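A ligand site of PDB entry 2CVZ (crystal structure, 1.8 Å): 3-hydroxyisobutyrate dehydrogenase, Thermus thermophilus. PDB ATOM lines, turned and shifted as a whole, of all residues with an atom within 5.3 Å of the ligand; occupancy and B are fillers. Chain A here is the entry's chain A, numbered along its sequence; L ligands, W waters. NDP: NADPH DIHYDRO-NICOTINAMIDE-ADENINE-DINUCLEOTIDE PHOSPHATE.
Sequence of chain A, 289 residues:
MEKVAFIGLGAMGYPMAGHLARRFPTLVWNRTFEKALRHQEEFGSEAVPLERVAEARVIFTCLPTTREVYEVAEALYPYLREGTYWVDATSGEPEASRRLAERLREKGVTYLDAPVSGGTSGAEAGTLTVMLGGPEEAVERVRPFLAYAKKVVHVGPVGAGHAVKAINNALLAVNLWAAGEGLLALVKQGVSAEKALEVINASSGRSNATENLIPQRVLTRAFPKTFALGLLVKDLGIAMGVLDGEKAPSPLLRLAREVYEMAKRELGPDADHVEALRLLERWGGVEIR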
ATOM      1  N   GLY A   8      -1.677  -9.226  22.724  1.00  0.00           N
ATOM      2  CA  GLY A   8      -2.789  -8.286  22.793  1.00  0.00           C
ATOM      3  C   GLY A   8      -3.620  -8.293  21.529  1.00  0.00           C
ATOM      4  O   GLY A   8      -3.473  -7.408  20.674  1.00  0.00           O
ATOM      5  N   LEU A   9      -4.487  -9.280  21.402  1.00  0.00           N
ATOM      6  CA  LEU A   9      -5.319  -9.396  20.210  1.00  0.00           C
ATOM      7  C   LEU A   9      -6.656  -8.699  20.407  1.00  0.00           C
ATOM      8  O   LEU A   9      -7.707  -9.338  20.415  1.00  0.00           O
ATOM      9  CB  LEU A   9      -5.540 -10.879  19.882  1.00  0.00           C
ATOM     10  CG  LEU A   9      -4.250 -11.682  19.731  1.00  0.00           C
ATOM     11  CD1 LEU A   9      -4.587 -13.150  19.482  1.00  0.00           C
ATOM     12  CD2 LEU A   9      -3.427 -11.115  18.574  1.00  0.00           C
ATOM     13  N   GLY A  10      -6.600  -7.373  20.544  1.00  0.00           N
ATOM     14  CA  GLY A  10      -7.818  -6.598  20.736  1.00  0.00           C
ATOM     15  C   GLY A  10      -8.370  -6.077  19.435  1.00  0.00           C
ATOM     16  O   GLY A  10      -8.096  -6.616  18.361  1.00  0.00           O
ATOM     17  N   ALA A  11      -9.183  -5.019  19.518  1.00  0.00           N
ATOM     18  CA  ALA A  11      -9.784  -4.425  18.330  1.00  0.00           C
ATOM     19  C   ALA A  11      -8.717  -4.123  17.287  1.00  0.00           C
ATOM     20  O   ALA A  11      -8.924  -4.325  16.097  1.00  0.00           O
ATOM     21  CB  ALA A  11     -10.534  -3.161  18.707  1.00  0.00           C
ATOM     22  N   MET A  12      -7.571  -3.633  17.752  1.00  0.00           N
ATOM     23  CA  MET A  12      -6.476  -3.301  16.855  1.00  0.00           C
ATOM     24  C   MET A  12      -5.532  -4.480  16.654  1.00  0.00           C
ATOM     25  O   MET A  12      -5.185  -4.827  15.523  1.00  0.00           O
ATOM     26  CB  MET A  12      -5.689  -2.120  17.398  1.00  0.00           C
ATOM     27  CG  MET A  12      -6.477  -0.827  17.452  1.00  0.00           C
ATOM     28  SD  MET A  12      -6.996  -0.219  15.681  1.00  0.00           S
ATOM     29  CE  MET A  12      -5.261   0.355  15.064  1.00  0.00           C
ATOM     30  N   GLY A  13      -5.116  -5.089  17.761  1.00  0.00           N
ATOM     31  CA  GLY A  13      -4.179  -6.203  17.718  1.00  0.00           C
ATOM     32  C   GLY A  13      -4.573  -7.425  16.911  1.00  0.00           C
ATOM     33  O   GLY A  13      -3.722  -8.013  16.246  1.00  0.00           O
ATOM     34  N   TRP A  29      -0.477 -14.478  21.433  1.00  0.00           N
ATOM     35  CA  TRP A  29      -0.936 -14.728  22.787  1.00  0.00           C
ATOM     36  C   TRP A  29      -1.907 -13.625  23.183  1.00  0.00           C
ATOM     37  O   TRP A  29      -1.758 -12.473  22.760  1.00  0.00           O
ATOM     38  CB  TRP A  29       0.230 -14.721  23.771  1.00  0.00           C
ATOM     39  CG  TRP A  29      -0.200 -14.922  25.197  1.00  0.00           C
ATOM     40  CD1 TRP A  29      -0.367 -16.109  25.850  1.00  0.00           C
ATOM     41  CD2 TRP A  29      -0.552 -13.893  26.145  1.00  0.00           C
ATOM     42  NE1 TRP A  29      -0.796 -15.892  27.147  1.00  0.00           N
ATOM     43  CE2 TRP A  29      -0.916 -14.541  27.352  1.00  0.00           C
ATOM     44  CE3 TRP A  29      -0.589 -12.493  26.090  1.00  0.00           C
ATOM     45  CZ2 TRP A  29      -1.317 -13.837  28.493  1.00  0.00           C
ATOM     46  CZ3 TRP A  29      -0.990 -11.789  27.231  1.00  0.00           C
ATOM     47  CH2 TRP A  29      -1.357 -12.460  28.414  1.00  0.00           C
ATOM     48  N   ASN A  30      -2.913 -13.980  23.969  1.00  0.00           N
ATOM     49  CA  ASN A  30      -3.887 -13.016  24.467  1.00  0.00           C
ATOM     50  C   ASN A  30      -4.301 -13.472  25.848  1.00  0.00           C
ATOM     51  O   ASN A  30      -4.400 -14.676  26.109  1.00  0.00           O
ATOM     52  CB  ASN A  30      -5.112 -12.952  23.552  1.00  0.00           C
ATOM     53  CG  ASN A  30      -5.997 -11.743  23.869  1.00  0.00           C
ATOM     54  OD1 ASN A  30      -5.561 -10.600  23.750  1.00  0.00           O
ATOM     55  ND2 ASN A  30      -7.238 -11.998  24.272  1.00  0.00           N
ATOM     56  N   ARG A  31      -4.531 -12.512  26.744  1.00  0.00           N
ATOM     57  CA  ARG A  31      -4.954 -12.796  28.111  1.00  0.00           C
ATOM     58  C   ARG A  31      -6.173 -13.713  28.071  1.00  0.00           C
ATOM     59  O   ARG A  31      -6.197 -14.747  28.753  1.00  0.00           O
ATOM     60  CB  ARG A  31      -5.290 -11.494  28.838  1.00  0.00           C
ATOM     61  CG  ARG A  31      -5.841 -11.706  30.222  1.00  0.00           C
ATOM     62  CD  ARG A  31      -6.112 -10.389  30.918  1.00  0.00           C
ATOM     63  NE  ARG A  31      -7.041  -9.558  30.153  1.00  0.00           N
ATOM     64  CZ  ARG A  31      -7.540  -8.402  30.594  1.00  0.00           C
ATOM     65  NH1 ARG A  31      -7.199  -7.957  31.793  1.00  0.00           N
ATOM     66  NH2 ARG A  31      -8.383  -7.714  29.837  1.00  0.00           N
ATOM     67  N   THR A  32      -7.188 -13.327  27.307  1.00  0.00           N
ATOM     68  CA  THR A  32      -8.396 -14.155  27.125  1.00  0.00           C
ATOM     69  C   THR A  32      -7.959 -15.003  25.931  1.00  0.00           C
ATOM     70  O   THR A  32      -8.117 -14.616  24.769  1.00  0.00           O
ATOM     71  CB  THR A  32      -9.610 -13.293  26.762  1.00  0.00           C
ATOM     72  OG1 THR A  32      -9.859 -12.370  27.814  1.00  0.00           O
ATOM     73  CG2 THR A  32     -10.841 -14.164  26.566  1.00  0.00           C
ATOM     74  N   LYS A  35      -9.222 -15.843  22.077  1.00  0.00           N
ATOM     75  CA  LYS A  35      -8.921 -14.948  20.957  1.00  0.00           C
ATOM     76  C   LYS A  35      -7.714 -15.441  20.176  1.00  0.00           C
ATOM     77  O   LYS A  35      -7.683 -15.337  18.942  1.00  0.00           O
ATOM     78  CB  LYS A  35      -8.663 -13.526  21.450  1.00  0.00           C
ATOM     79  CG  LYS A  35      -9.893 -12.817  22.012  1.00  0.00           C
ATOM     80  CD  LYS A  35     -10.965 -12.612  20.938  1.00  0.00           C
ATOM     81  CE  LYS A  35     -12.158 -11.828  21.464  1.00  0.00           C
ATOM     82  NZ  LYS A  35     -11.792 -10.438  21.865  1.00  0.00           N
ATOM     83  N   CYS A  62       0.068  -4.531  21.769  1.00  0.00           N
ATOM     84  CA  CYS A  62      -0.936  -3.498  21.502  1.00  0.00           C
ATOM     85  C   CYS A  62      -1.939  -3.665  22.624  1.00  0.00           C
ATOM     86  O   CYS A  62      -2.985  -4.301  22.477  1.00  0.00           O
ATOM     87  CB  CYS A  62      -1.621  -3.689  20.146  1.00  0.00           C
ATOM     88  SG  CYS A  62      -2.609  -2.234  19.664  1.00  0.00           S
ATOM     89  N   LEU A  63      -1.574  -3.107  23.774  1.00  0.00           N
ATOM     90  CA  LEU A  63      -2.363  -3.189  24.999  1.00  0.00           C
ATOM     91  C   LEU A  63      -3.019  -1.841  25.318  1.00  0.00           C
ATOM     92  O   LEU A  63      -2.784  -0.856  24.625  1.00  0.00           O
ATOM     93  CB  LEU A  63      -1.430  -3.652  26.127  1.00  0.00           C
ATOM     94  CG  LEU A  63      -0.770  -4.995  25.791  1.00  0.00           C
ATOM     95  CD1 LEU A  63       0.374  -5.310  26.762  1.00  0.00           C
ATOM     96  CD2 LEU A  63      -1.820  -6.093  25.823  1.00  0.00           C
ATOM     97  N   PRO A  64      -3.852  -1.790  26.368  1.00  0.00           N
ATOM     98  CA  PRO A  64      -4.511  -0.535  26.727  1.00  0.00           C
ATOM     99  C   PRO A  64      -3.569   0.609  27.068  1.00  0.00           C
ATOM    100  O   PRO A  64      -3.655   1.685  26.473  1.00  0.00           O
ATOM    101  CB  PRO A  64      -5.377  -0.934  27.916  1.00  0.00           C
ATOM    102  CG  PRO A  64      -5.724  -2.363  27.613  1.00  0.00           C
ATOM    103  CD  PRO A  64      -4.387  -2.903  27.166  1.00  0.00           C
ATOM    104  N   THR A  65      -2.685   0.374  28.034  1.00  0.00           N
ATOM    105  CA  THR A  65      -1.742   1.401  28.476  1.00  0.00           C
ATOM    106  C   THR A  65      -0.377   0.810  28.786  1.00  0.00           C
ATOM    107  O   THR A  65      -0.210  -0.402  28.832  1.00  0.00           O
ATOM    108  CB  THR A  65      -2.233   2.096  29.758  1.00  0.00           C
ATOM    109  OG1 THR A  65      -2.146   1.178  30.858  1.00  0.00           O
ATOM    110  CG2 THR A  65      -3.683   2.536  29.615  1.00  0.00           C
ATOM    111  N   GLU A  68      -0.045  -2.063  31.345  1.00  0.00           N
ATOM    112  CA  GLU A  68      -0.187  -3.459  30.927  1.00  0.00           C
ATOM    113  C   GLU A  68       1.043  -3.949  30.169  1.00  0.00           C
ATOM    114  O   GLU A  68       1.361  -5.140  30.224  1.00  0.00           O
ATOM    115  CB  GLU A  68      -1.429  -3.660  30.066  1.00  0.00           C
ATOM    116  CG  GLU A  68      -2.766  -3.506  30.800  1.00  0.00           C
ATOM    117  CD  GLU A  68      -3.080  -2.058  31.158  1.00  0.00           C
ATOM    118  OE1 GLU A  68      -2.870  -1.179  30.297  1.00  0.00           O
ATOM    119  OE2 GLU A  68      -3.553  -1.815  32.287  1.00  0.00           O
ATOM    120  N   GLU A  71       3.354  -5.056  32.801  1.00  0.00           N
ATOM    121  CA  GLU A  71       2.934  -6.337  33.365  1.00  0.00           C
ATOM    122  C   GLU A  71       3.435  -7.486  32.503  1.00  0.00           C
ATOM    123  O   GLU A  71       3.985  -8.459  33.019  1.00  0.00           O
ATOM    124  CB  GLU A  71       1.402  -6.416  33.462  1.00  0.00           C
ATOM    125  CG  GLU A  71       0.753  -5.295  34.254  1.00  0.00           C
ATOM    126  CD  GLU A  71      -0.751  -5.465  34.387  1.00  0.00           C
ATOM    127  OE1 GLU A  71      -1.419  -4.508  34.826  1.00  0.00           O
ATOM    128  OE2 GLU A  71      -1.266  -6.563  34.044  1.00  0.00           O
ATOM    129  N   VAL A  72       3.231  -7.387  31.196  1.00  0.00           N
ATOM    130  CA  VAL A  72       3.662  -8.428  30.275  1.00  0.00           C
ATOM    131  C   VAL A  72       5.190  -8.532  30.217  1.00  0.00           C
ATOM    132  O   VAL A  72       5.748  -9.633  30.193  1.00  0.00           O
ATOM    133  CB  VAL A  72       3.102  -8.175  28.860  1.00  0.00           C
ATOM    134  CG1 VAL A  72       3.680  -9.169  27.885  1.00  0.00           C
ATOM    135  CG2 VAL A  72       1.590  -8.285  28.889  1.00  0.00           C
ATOM    136  N   ALA A  89       3.025  -1.074  19.996  1.00  0.00           N
ATOM    137  CA  ALA A  89       1.985  -0.342  19.283  1.00  0.00           C
ATOM    138  C   ALA A  89       0.924   0.219  20.214  1.00  0.00           C
ATOM    139  O   ALA A  89      -0.098   0.752  19.776  1.00  0.00           O
ATOM    140  CB  ALA A  89       1.329  -1.240  18.237  1.00  0.00           C
ATOM    141  N   THR A  90       1.155   0.077  21.517  1.00  0.00           N
ATOM    142  CA  THR A  90       0.251   0.606  22.532  1.00  0.00           C
ATOM    143  C   THR A  90       0.348   2.141  22.444  1.00  0.00           C
ATOM    144  O   THR A  90       1.408   2.664  22.130  1.00  0.00           O
ATOM    145  CB  THR A  90       0.728   0.191  23.954  1.00  0.00           C
ATOM    146  OG1 THR A  90       0.670  -1.233  24.073  1.00  0.00           O
ATOM    147  CG2 THR A  90      -0.128   0.849  25.036  1.00  0.00           C
ATOM    148  N   SER A  91      -0.749   2.847  22.697  1.00  0.00           N
ATOM    149  CA  SER A  91      -0.665   4.310  22.718  1.00  0.00           C
ATOM    150  C   SER A  91      -0.219   4.524  24.152  1.00  0.00           C
ATOM    151  O   SER A  91      -1.029   4.636  25.069  1.00  0.00           O
ATOM    152  CB  SER A  91      -2.041   4.932  22.474  1.00  0.00           C
ATOM    153  OG  SER A  91      -2.387   4.809  21.112  1.00  0.00           O
ATOM    154  N   VAL A 116       0.072   3.607  16.516  1.00  0.00           N
ATOM    155  CA  VAL A 116      -0.494   3.674  15.182  1.00  0.00           C
ATOM    156  C   VAL A 116      -1.759   4.519  15.070  1.00  0.00           C
ATOM    157  O   VAL A 116      -2.394   4.837  16.070  1.00  0.00           O
ATOM    158  CB  VAL A 116      -0.851   2.253  14.691  1.00  0.00           C
ATOM    159  CG1 VAL A 116       0.387   1.370  14.662  1.00  0.00           C
ATOM    160  CG2 VAL A 116      -1.895   1.643  15.625  1.00  0.00           C
ATOM    161  N   SER A 117      -2.098   4.864  13.840  1.00  0.00           N
ATOM    162  CA  SER A 117      -3.316   5.613  13.566  1.00  0.00           C
ATOM    163  C   SER A 117      -3.948   5.046  12.300  1.00  0.00           C
ATOM    164  O   SER A 117      -3.246   4.625  11.372  1.00  0.00           O
ATOM    165  CB  SER A 117      -3.023   7.091  13.366  1.00  0.00           C
ATOM    166  OG  SER A 117      -4.241   7.823  13.241  1.00  0.00           O
ATOM    167  N   GLY A 119      -7.369   3.508  12.865  1.00  0.00           N
ATOM    168  CA  GLY A 119      -8.523   2.814  13.400  1.00  0.00           C
ATOM    169  C   GLY A 119      -8.612   1.351  13.015  1.00  0.00           C
ATOM    170  O   GLY A 119      -7.693   0.811  12.388  1.00  0.00           O
ATOM    171  N   THR A 120      -9.692   0.688  13.392  1.00  0.00           N
ATOM    172  CA  THR A 120      -9.857  -0.720  13.068  1.00  0.00           C
ATOM    173  C   THR A 120      -9.966  -0.957  11.555  1.00  0.00           C
ATOM    174  O   THR A 120      -9.618  -2.045  11.082  1.00  0.00           O
ATOM    175  CB  THR A 120     -11.096  -1.337  13.758  1.00  0.00           C
ATOM    176  OG1 THR A 120     -12.267  -0.582  13.418  1.00  0.00           O
ATOM    177  CG2 THR A 120     -10.917  -1.349  15.270  1.00  0.00           C
ATOM    178  N   LYS A 165       1.628  10.504  18.917  1.00  0.00           N
ATOM    179  CA  LYS A 165       0.325   9.853  18.890  1.00  0.00           C
ATOM    180  C   LYS A 165      -0.657  10.563  19.810  1.00  0.00           C
ATOM    181  O   LYS A 165      -1.807  10.820  19.430  1.00  0.00           O
ATOM    182  CB  LYS A 165       0.451   8.386  19.338  1.00  0.00           C
ATOM    183  CG  LYS A 165      -0.894   7.666  19.523  1.00  0.00           C
ATOM    184  CD  LYS A 165      -1.696   7.539  18.233  1.00  0.00           C
ATOM    185  CE  LYS A 165      -3.013   6.797  18.504  1.00  0.00           C
ATOM    186  NZ  LYS A 165      -3.943   6.804  17.335  1.00  0.00           N
ATOM    187  N   THR A 226     -15.565   0.858  17.779  1.00  0.00           N
ATOM    188  CA  THR A 226     -14.247   0.498  17.244  1.00  0.00           C
ATOM    189  C   THR A 226     -13.102   1.042  18.095  1.00  0.00           C
ATOM    190  O   THR A 226     -12.007   0.506  18.078  1.00  0.00           O
ATOM    191  CB  THR A 226     -14.050   0.996  15.792  1.00  0.00           C
ATOM    192  OG1 THR A 226     -13.895   2.419  15.785  1.00  0.00           O
ATOM    193  CG2 THR A 226     -15.238   0.608  14.928  1.00  0.00           C
ATOM    194  N   PHE A 227     -13.356   2.107  18.844  1.00  0.00           N
ATOM    195  CA  PHE A 227     -12.325   2.717  19.696  1.00  0.00           C
ATOM    196  C   PHE A 227     -13.015   3.283  20.942  1.00  0.00           C
ATOM    197  O   PHE A 227     -13.757   4.260  20.867  1.00  0.00           O
ATOM    198  CB  PHE A 227     -11.615   3.835  18.915  1.00  0.00           C
ATOM    199  CG  PHE A 227     -10.582   4.595  19.708  1.00  0.00           C
ATOM    200  CD1 PHE A 227      -9.699   3.929  20.545  1.00  0.00           C
ATOM    201  CD2 PHE A 227     -10.480   5.974  19.576  1.00  0.00           C
ATOM    202  CE1 PHE A 227      -8.713   4.632  21.255  1.00  0.00           C
ATOM    203  CE2 PHE A 227      -9.499   6.683  20.274  1.00  0.00           C
ATOM    204  CZ  PHE A 227      -8.615   6.007  21.116  1.00  0.00           C
ATOM    205  N   ALA A 228     -12.762   2.651  22.085  1.00  0.00           N
ATOM    206  CA  ALA A 228     -13.376   3.043  23.348  1.00  0.00           C
ATOM    207  C   ALA A 228     -13.164   4.499  23.759  1.00  0.00           C
ATOM    208  O   ALA A 228     -12.046   5.004  23.713  1.00  0.00           O
ATOM    209  CB  ALA A 228     -12.892   2.122  24.464  1.00  0.00           C
ATOM    210  N   LEU A 231     -10.490   5.001  26.258  1.00  0.00           N
ATOM    211  CA  LEU A 231      -9.113   5.000  25.758  1.00  0.00           C
ATOM    212  C   LEU A 231      -8.760   6.364  25.172  1.00  0.00           C
ATOM    213  O   LEU A 231      -7.620   6.823  25.279  1.00  0.00           O
ATOM    214  CB  LEU A 231      -8.910   3.910  24.696  1.00  0.00           C
ATOM    215  CG  LEU A 231      -8.978   2.460  25.201  1.00  0.00           C
ATOM    216  CD1 LEU A 231      -8.926   1.498  24.024  1.00  0.00           C
ATOM    217  CD2 LEU A 231      -7.813   2.196  26.157  1.00  0.00           C
ATOM    218  N   LYS A 234      -7.959   8.497  27.909  1.00  0.00           N
ATOM    219  CA  LYS A 234      -6.632   8.118  28.388  1.00  0.00           C
ATOM    220  C   LYS A 234      -5.574   8.783  27.517  1.00  0.00           C
ATOM    221  O   LYS A 234      -4.563   9.279  28.025  1.00  0.00           O
ATOM    222  CB  LYS A 234      -6.490   6.591  28.368  1.00  0.00           C
ATOM    223  CG  LYS A 234      -5.070   6.064  28.613  1.00  0.00           C
ATOM    224  CD  LYS A 234      -4.278   5.908  27.314  1.00  0.00           C
ATOM    225  CE  LYS A 234      -4.861   4.815  26.424  1.00  0.00           C
ATOM    226  NZ  LYS A 234      -4.123   4.657  25.131  1.00  0.00           N
ATOM    227  N   ASP A 235      -5.783   8.788  26.201  1.00  0.00           N
ATOM    228  CA  ASP A 235      -4.844   9.423  25.272  1.00  0.00           C
ATOM    229  C   ASP A 235      -4.784  10.924  25.538  1.00  0.00           C
ATOM    230  O   ASP A 235      -3.708  11.528  25.498  1.00  0.00           O
ATOM    231  CB  ASP A 235      -5.265   9.223  23.817  1.00  0.00           C
ATOM    232  CG  ASP A 235      -5.153   7.792  23.358  1.00  0.00           C
ATOM    233  OD1 ASP A 235      -4.277   7.074  23.886  1.00  0.00           O
ATOM    234  OD2 ASP A 235      -5.922   7.392  22.465  1.00  0.00           O
HETATM  235  PA  NDP L   1      -9.094  -3.415  23.167  1.00  0.00           P
HETATM  236  O1A NDP L   1      -9.887  -3.901  22.057  1.00  0.00           O
HETATM  237  O2A NDP L   1      -9.677  -3.001  24.489  1.00  0.00           O
HETATM  238  O5B NDP L   1      -7.952  -4.570  23.427  1.00  0.00           O
HETATM  239  C5B NDP L   1      -7.015  -4.400  24.520  1.00  0.00           C
HETATM  240  C4B NDP L   1      -6.143  -5.648  24.446  1.00  0.00           C
HETATM  241  O4B NDP L   1      -5.220  -5.552  25.575  1.00  0.00           O
HETATM  242  C3B NDP L   1      -6.831  -6.973  24.548  1.00  0.00           C
HETATM  243  O3B NDP L   1      -6.122  -7.935  23.724  1.00  0.00           O
HETATM  244  C2B NDP L   1      -6.713  -7.347  25.976  1.00  0.00           C
HETATM  245  O2B NDP L   1      -6.924  -8.711  26.346  1.00  0.00           O
HETATM  246  C1B NDP L   1      -5.378  -6.769  26.303  1.00  0.00           C
HETATM  247  N9A NDP L   1      -5.183  -6.546  27.766  1.00  0.00           N
HETATM  248  C8A NDP L   1      -5.903  -5.685  28.639  1.00  0.00           C
HETATM  249  N7A NDP L   1      -5.443  -5.759  29.869  1.00  0.00           N
HETATM  250  C5A NDP L   1      -4.417  -6.674  29.846  1.00  0.00           C
HETATM  251  C6A NDP L   1      -3.541  -7.196  30.821  1.00  0.00           C
HETATM  252  N6A NDP L   1      -3.618  -6.777  32.083  1.00  0.00           N
HETATM  253  N1A NDP L   1      -2.610  -8.110  30.457  1.00  0.00           N
HETATM  254  C2A NDP L   1      -2.533  -8.529  29.170  1.00  0.00           C
HETATM  255  N3A NDP L   1      -3.320  -8.098  28.171  1.00  0.00           N
HETATM  256  C4A NDP L   1      -4.252  -7.165  28.576  1.00  0.00           C
HETATM  257  O3  NDP L   1      -8.122  -2.271  22.698  1.00  0.00           O
HETATM  258  PN  NDP L   1      -7.777  -1.515  21.328  1.00  0.00           P
HETATM  259  O1N NDP L   1      -8.980  -0.793  20.884  1.00  0.00           O
HETATM  260  O2N NDP L   1      -7.186  -2.605  20.499  1.00  0.00           O
HETATM  261  O5D NDP L   1      -6.593  -0.557  21.805  1.00  0.00           O
HETATM  262  C5D NDP L   1      -5.286  -1.066  22.252  1.00  0.00           C
HETATM  263  C4D NDP L   1      -4.282   0.114  22.124  1.00  0.00           C
HETATM  264  O4D NDP L   1      -4.371   0.627  20.793  1.00  0.00           O
HETATM  265  C3D NDP L   1      -4.668   1.289  23.036  1.00  0.00           C
HETATM  266  O3D NDP L   1      -3.474   1.848  23.587  1.00  0.00           O
HETATM  267  C2D NDP L   1      -5.423   2.233  22.141  1.00  0.00           C
HETATM  268  O2D NDP L   1      -5.430   3.541  22.713  1.00  0.00           O
HETATM  269  C1D NDP L   1      -4.551   2.046  20.829  1.00  0.00           C
HETATM  270  N1N NDP L   1      -5.238   2.434  19.560  1.00  0.00           N
HETATM  271  C2N NDP L   1      -6.604   2.067  19.374  1.00  0.00           C
HETATM  272  C3N NDP L   1      -7.217   2.448  18.119  1.00  0.00           C
HETATM  273  C7N NDP L   1      -8.611   2.113  17.842  1.00  0.00           C
HETATM  274  O7N NDP L   1      -9.280   2.642  16.928  1.00  0.00           O
HETATM  275  N7N NDP L   1      -9.246   1.170  18.575  1.00  0.00           N
HETATM  276  C4N NDP L   1      -6.443   3.149  17.180  1.00  0.00           C
HETATM  277  C5N NDP L   1      -5.137   3.496  17.385  1.00  0.00           C
HETATM  278  C6N NDP L   1      -4.533   3.144  18.564  1.00  0.00           C
HETATM  279  P2B NDP L   1      -8.321  -9.353  26.541  1.00  0.00           P
HETATM  280  O1X NDP L   1      -8.047 -10.476  27.453  1.00  0.00           O
HETATM  281  O2X NDP L   1      -8.832  -9.790  25.215  1.00  0.00           O
HETATM  282  O3X NDP L   1      -9.272  -8.346  27.169  1.00  0.00           O
HETATM  283  O   HOH W   1      -9.380  -8.980  22.719  1.00  0.00           O
HETATM  284  O   HOH W   2      -5.440  -4.969  33.658  1.00  0.00           O
HETATM  285  O   HOH W   3     -10.967  -6.644  22.984  1.00  0.00           O
HETATM  286  O   HOH W   4     -11.622  -8.619  28.291  1.00  0.00           O
HETATM  287  O   HOH W   5     -10.229  -6.333  25.670  1.00  0.00           O
HETATM  288  O   HOH W   6      -3.691  -9.984  26.001  1.00  0.00           O
HETATM  289  O   HOH W   7     -11.188   0.093  21.849  1.00  0.00           O
HETATM  290  O   HOH W   8      -5.250  -4.675  20.696  1.00  0.00           O
HETATM  291  O   HOH W   9     -11.253 -10.386  24.549  1.00  0.00           O
HETATM  292  O   HOH W  10     -12.718  -3.639  22.048  1.00  0.00           O
HETATM  293  O   HOH W  11      -6.680  -3.887  31.486  1.00  0.00           O
HETATM  294  O   HOH W  12      -5.037   5.429  20.948  1.00  0.00           O
HETATM  295  O   HOH W  13     -11.268   2.496  15.251  1.00  0.00           O
HETATM  296  O   HOH W  14      -1.415 -10.246  31.832  1.00  0.00           O
HETATM  297  O   HOH W  15     -11.507  -1.053  24.315  1.00  0.00           O
HETATM  298  O   HOH W  16      -9.014   5.347  16.220  1.00  0.00           O
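The backbone NH (N) of Leu 9 is in hydrogen-bond range of an oxygen (O3B) of the ligand (3.1 Å). An oxygen (O3B) of the ligand sits at hydrogen-bond distance from the backbone NH of Gly 10 (3.3 Å). The backbone NH (N) of Ser 91 is in hydrogen-bond range of an oxygen (O3D) of the ligand (3.0 Å). The backbone carbonyl oxygen of Thr 226 lies within hydrogen-bond range of a nitrogen (N7N) of the ligand (2.9 Å). The backbone carbonyl oxygen (O) of Leu 63 is in hydrogen-bond range of an oxygen (O3D) of the ligand (3.0 Å). An oxygen (O3B) of the ligand sits at hydrogen-bond distance from the side-chain amide oxygen (OD1) of Asn 30, 2.7 Å away. The backbone NH (N) of Thr 32 lies within hydrogen-bond range of an oxygen (O1X) of the ligand, 3.0 Å away. NH2 of Arg 31 is in salt-bridge range of O3X of the ligand, at 2.9 Å. The backbone NH (N) of Met 12 sits at hydrogen-bond distance from an oxygen (O2N) of the ligand, at 3.0 Å. The side-chain sulfur of Cys 62 is in hydrogen-bond range of an oxygen (O4D) of the ligand, at 3.5 Å. O3D of the ligand lies within hydrogen-bond range of O of Pro 64 (2.9 Å). O2D of the ligand lies within hydrogen-bond range of NZ of Lys 234. The backbone NH (N) of Ala 11 sits at hydrogen-bond distance from an oxygen (O1A) of the ligand (2.9 Å). An oxygen (O1X) of the ligand is in hydrogen-bond range of the side-chain hydroxyl (OG1) of Thr 32 (2.6 Å). OE2 of Glu 71 lies within hydrogen-bond range of N6A of the ligand (3.1 Å).
The backbone NH (N) of Leu 63 is in hydrogen-bond range of the side-chain hydroxyl (OG1) of Thr 90, at 2.9 Å. O of Pro 64 lies within hydrogen-bond range of NZ of Lys 234 (3.3 Å). The backbone carbonyl oxygen of Ser 91 sits at hydrogen-bond distance from the side-chain amino group of Lys 234 (3.1 Å). The side-chain hydroxyl (OG1) of Thr 65 sits at hydrogen-bond distance from the side-chain carboxylate (OE1) of Glu 68 (2.5 Å). OD1 of Asn 30 sits at hydrogen-bond distance from N of Leu 9. N of Gly 8 is in hydrogen-bond range of O of Trp 29, 3.2 Å away. The backbone carbonyl oxygen (O) of Thr 32 lies within hydrogen-bond range of the side-chain amide nitrogen (ND2) of Asn 30 (2.8 Å). NZ of Lys 234 is in salt-bridge range of OD1 of Asp 235, 2.7 Å away.
Merely in contact with the ligand: Gly 8 (3.3 Å), Glu 68 (3.6 Å), Thr 90 (3.8 Å), Val 116 (3.3 Å), Gly 119 (3.6 Å), Lys 165 (3.5 Å), Phe 227 (3.3 Å), Leu 231 (3.8 Å) and Asp 235 (3.9 Å). Hydrophobic or aromatic side chains that line the ligand: Ala 11, Met 12, Leu 63, Pro 64, Phe 227 and Leu 231. Of the 32 residues printed, 23 come within 4 Å of the ligand. The nearest printed residue that does not touch the ligand is Thr 120 (4.1 Å).
Water W9 lies within hydrogen-bond range of O2X of the ligand (2.6 Å) and NZ of Lys 35 (2.7 Å). Water W13 lies within hydrogen-bond range of an oxygen (O7N) of the ligand (2.6 Å), the side-chain hydroxyl (OG1) of Thr 226 (2.7 Å) and the backbone NH (N) of Thr 120 (3.0 Å). Water W12 lies within hydrogen-bond range of O2D of the ligand (2.6 Å), OD2 of Asp 235 (2.6 Å) and OG of Ser 91 (2.7 Å). Water W1 lies within hydrogen-bond range of O2X of the ligand (2.7 Å), O of Leu 9 (2.9 Å) and NZ of Lys 35 (2.9 Å). Water W8 lies within hydrogen-bond range of O2N of the ligand (2.8 Å), O of Cys 62 (2.9 Å), N of Gly 13 (3.0 Å), N of Gly 10 (3.0 Å) and O of Gly 8 (3.3 Å). Water W6 lies within hydrogen-bond range of the backbone NH (N) of Arg 31 (2.8 Å), a nitrogen (N3A) of the ligand (2.9 Å) and the side-chain amide oxygen (OD1) of Asn 30 (3.0 Å).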
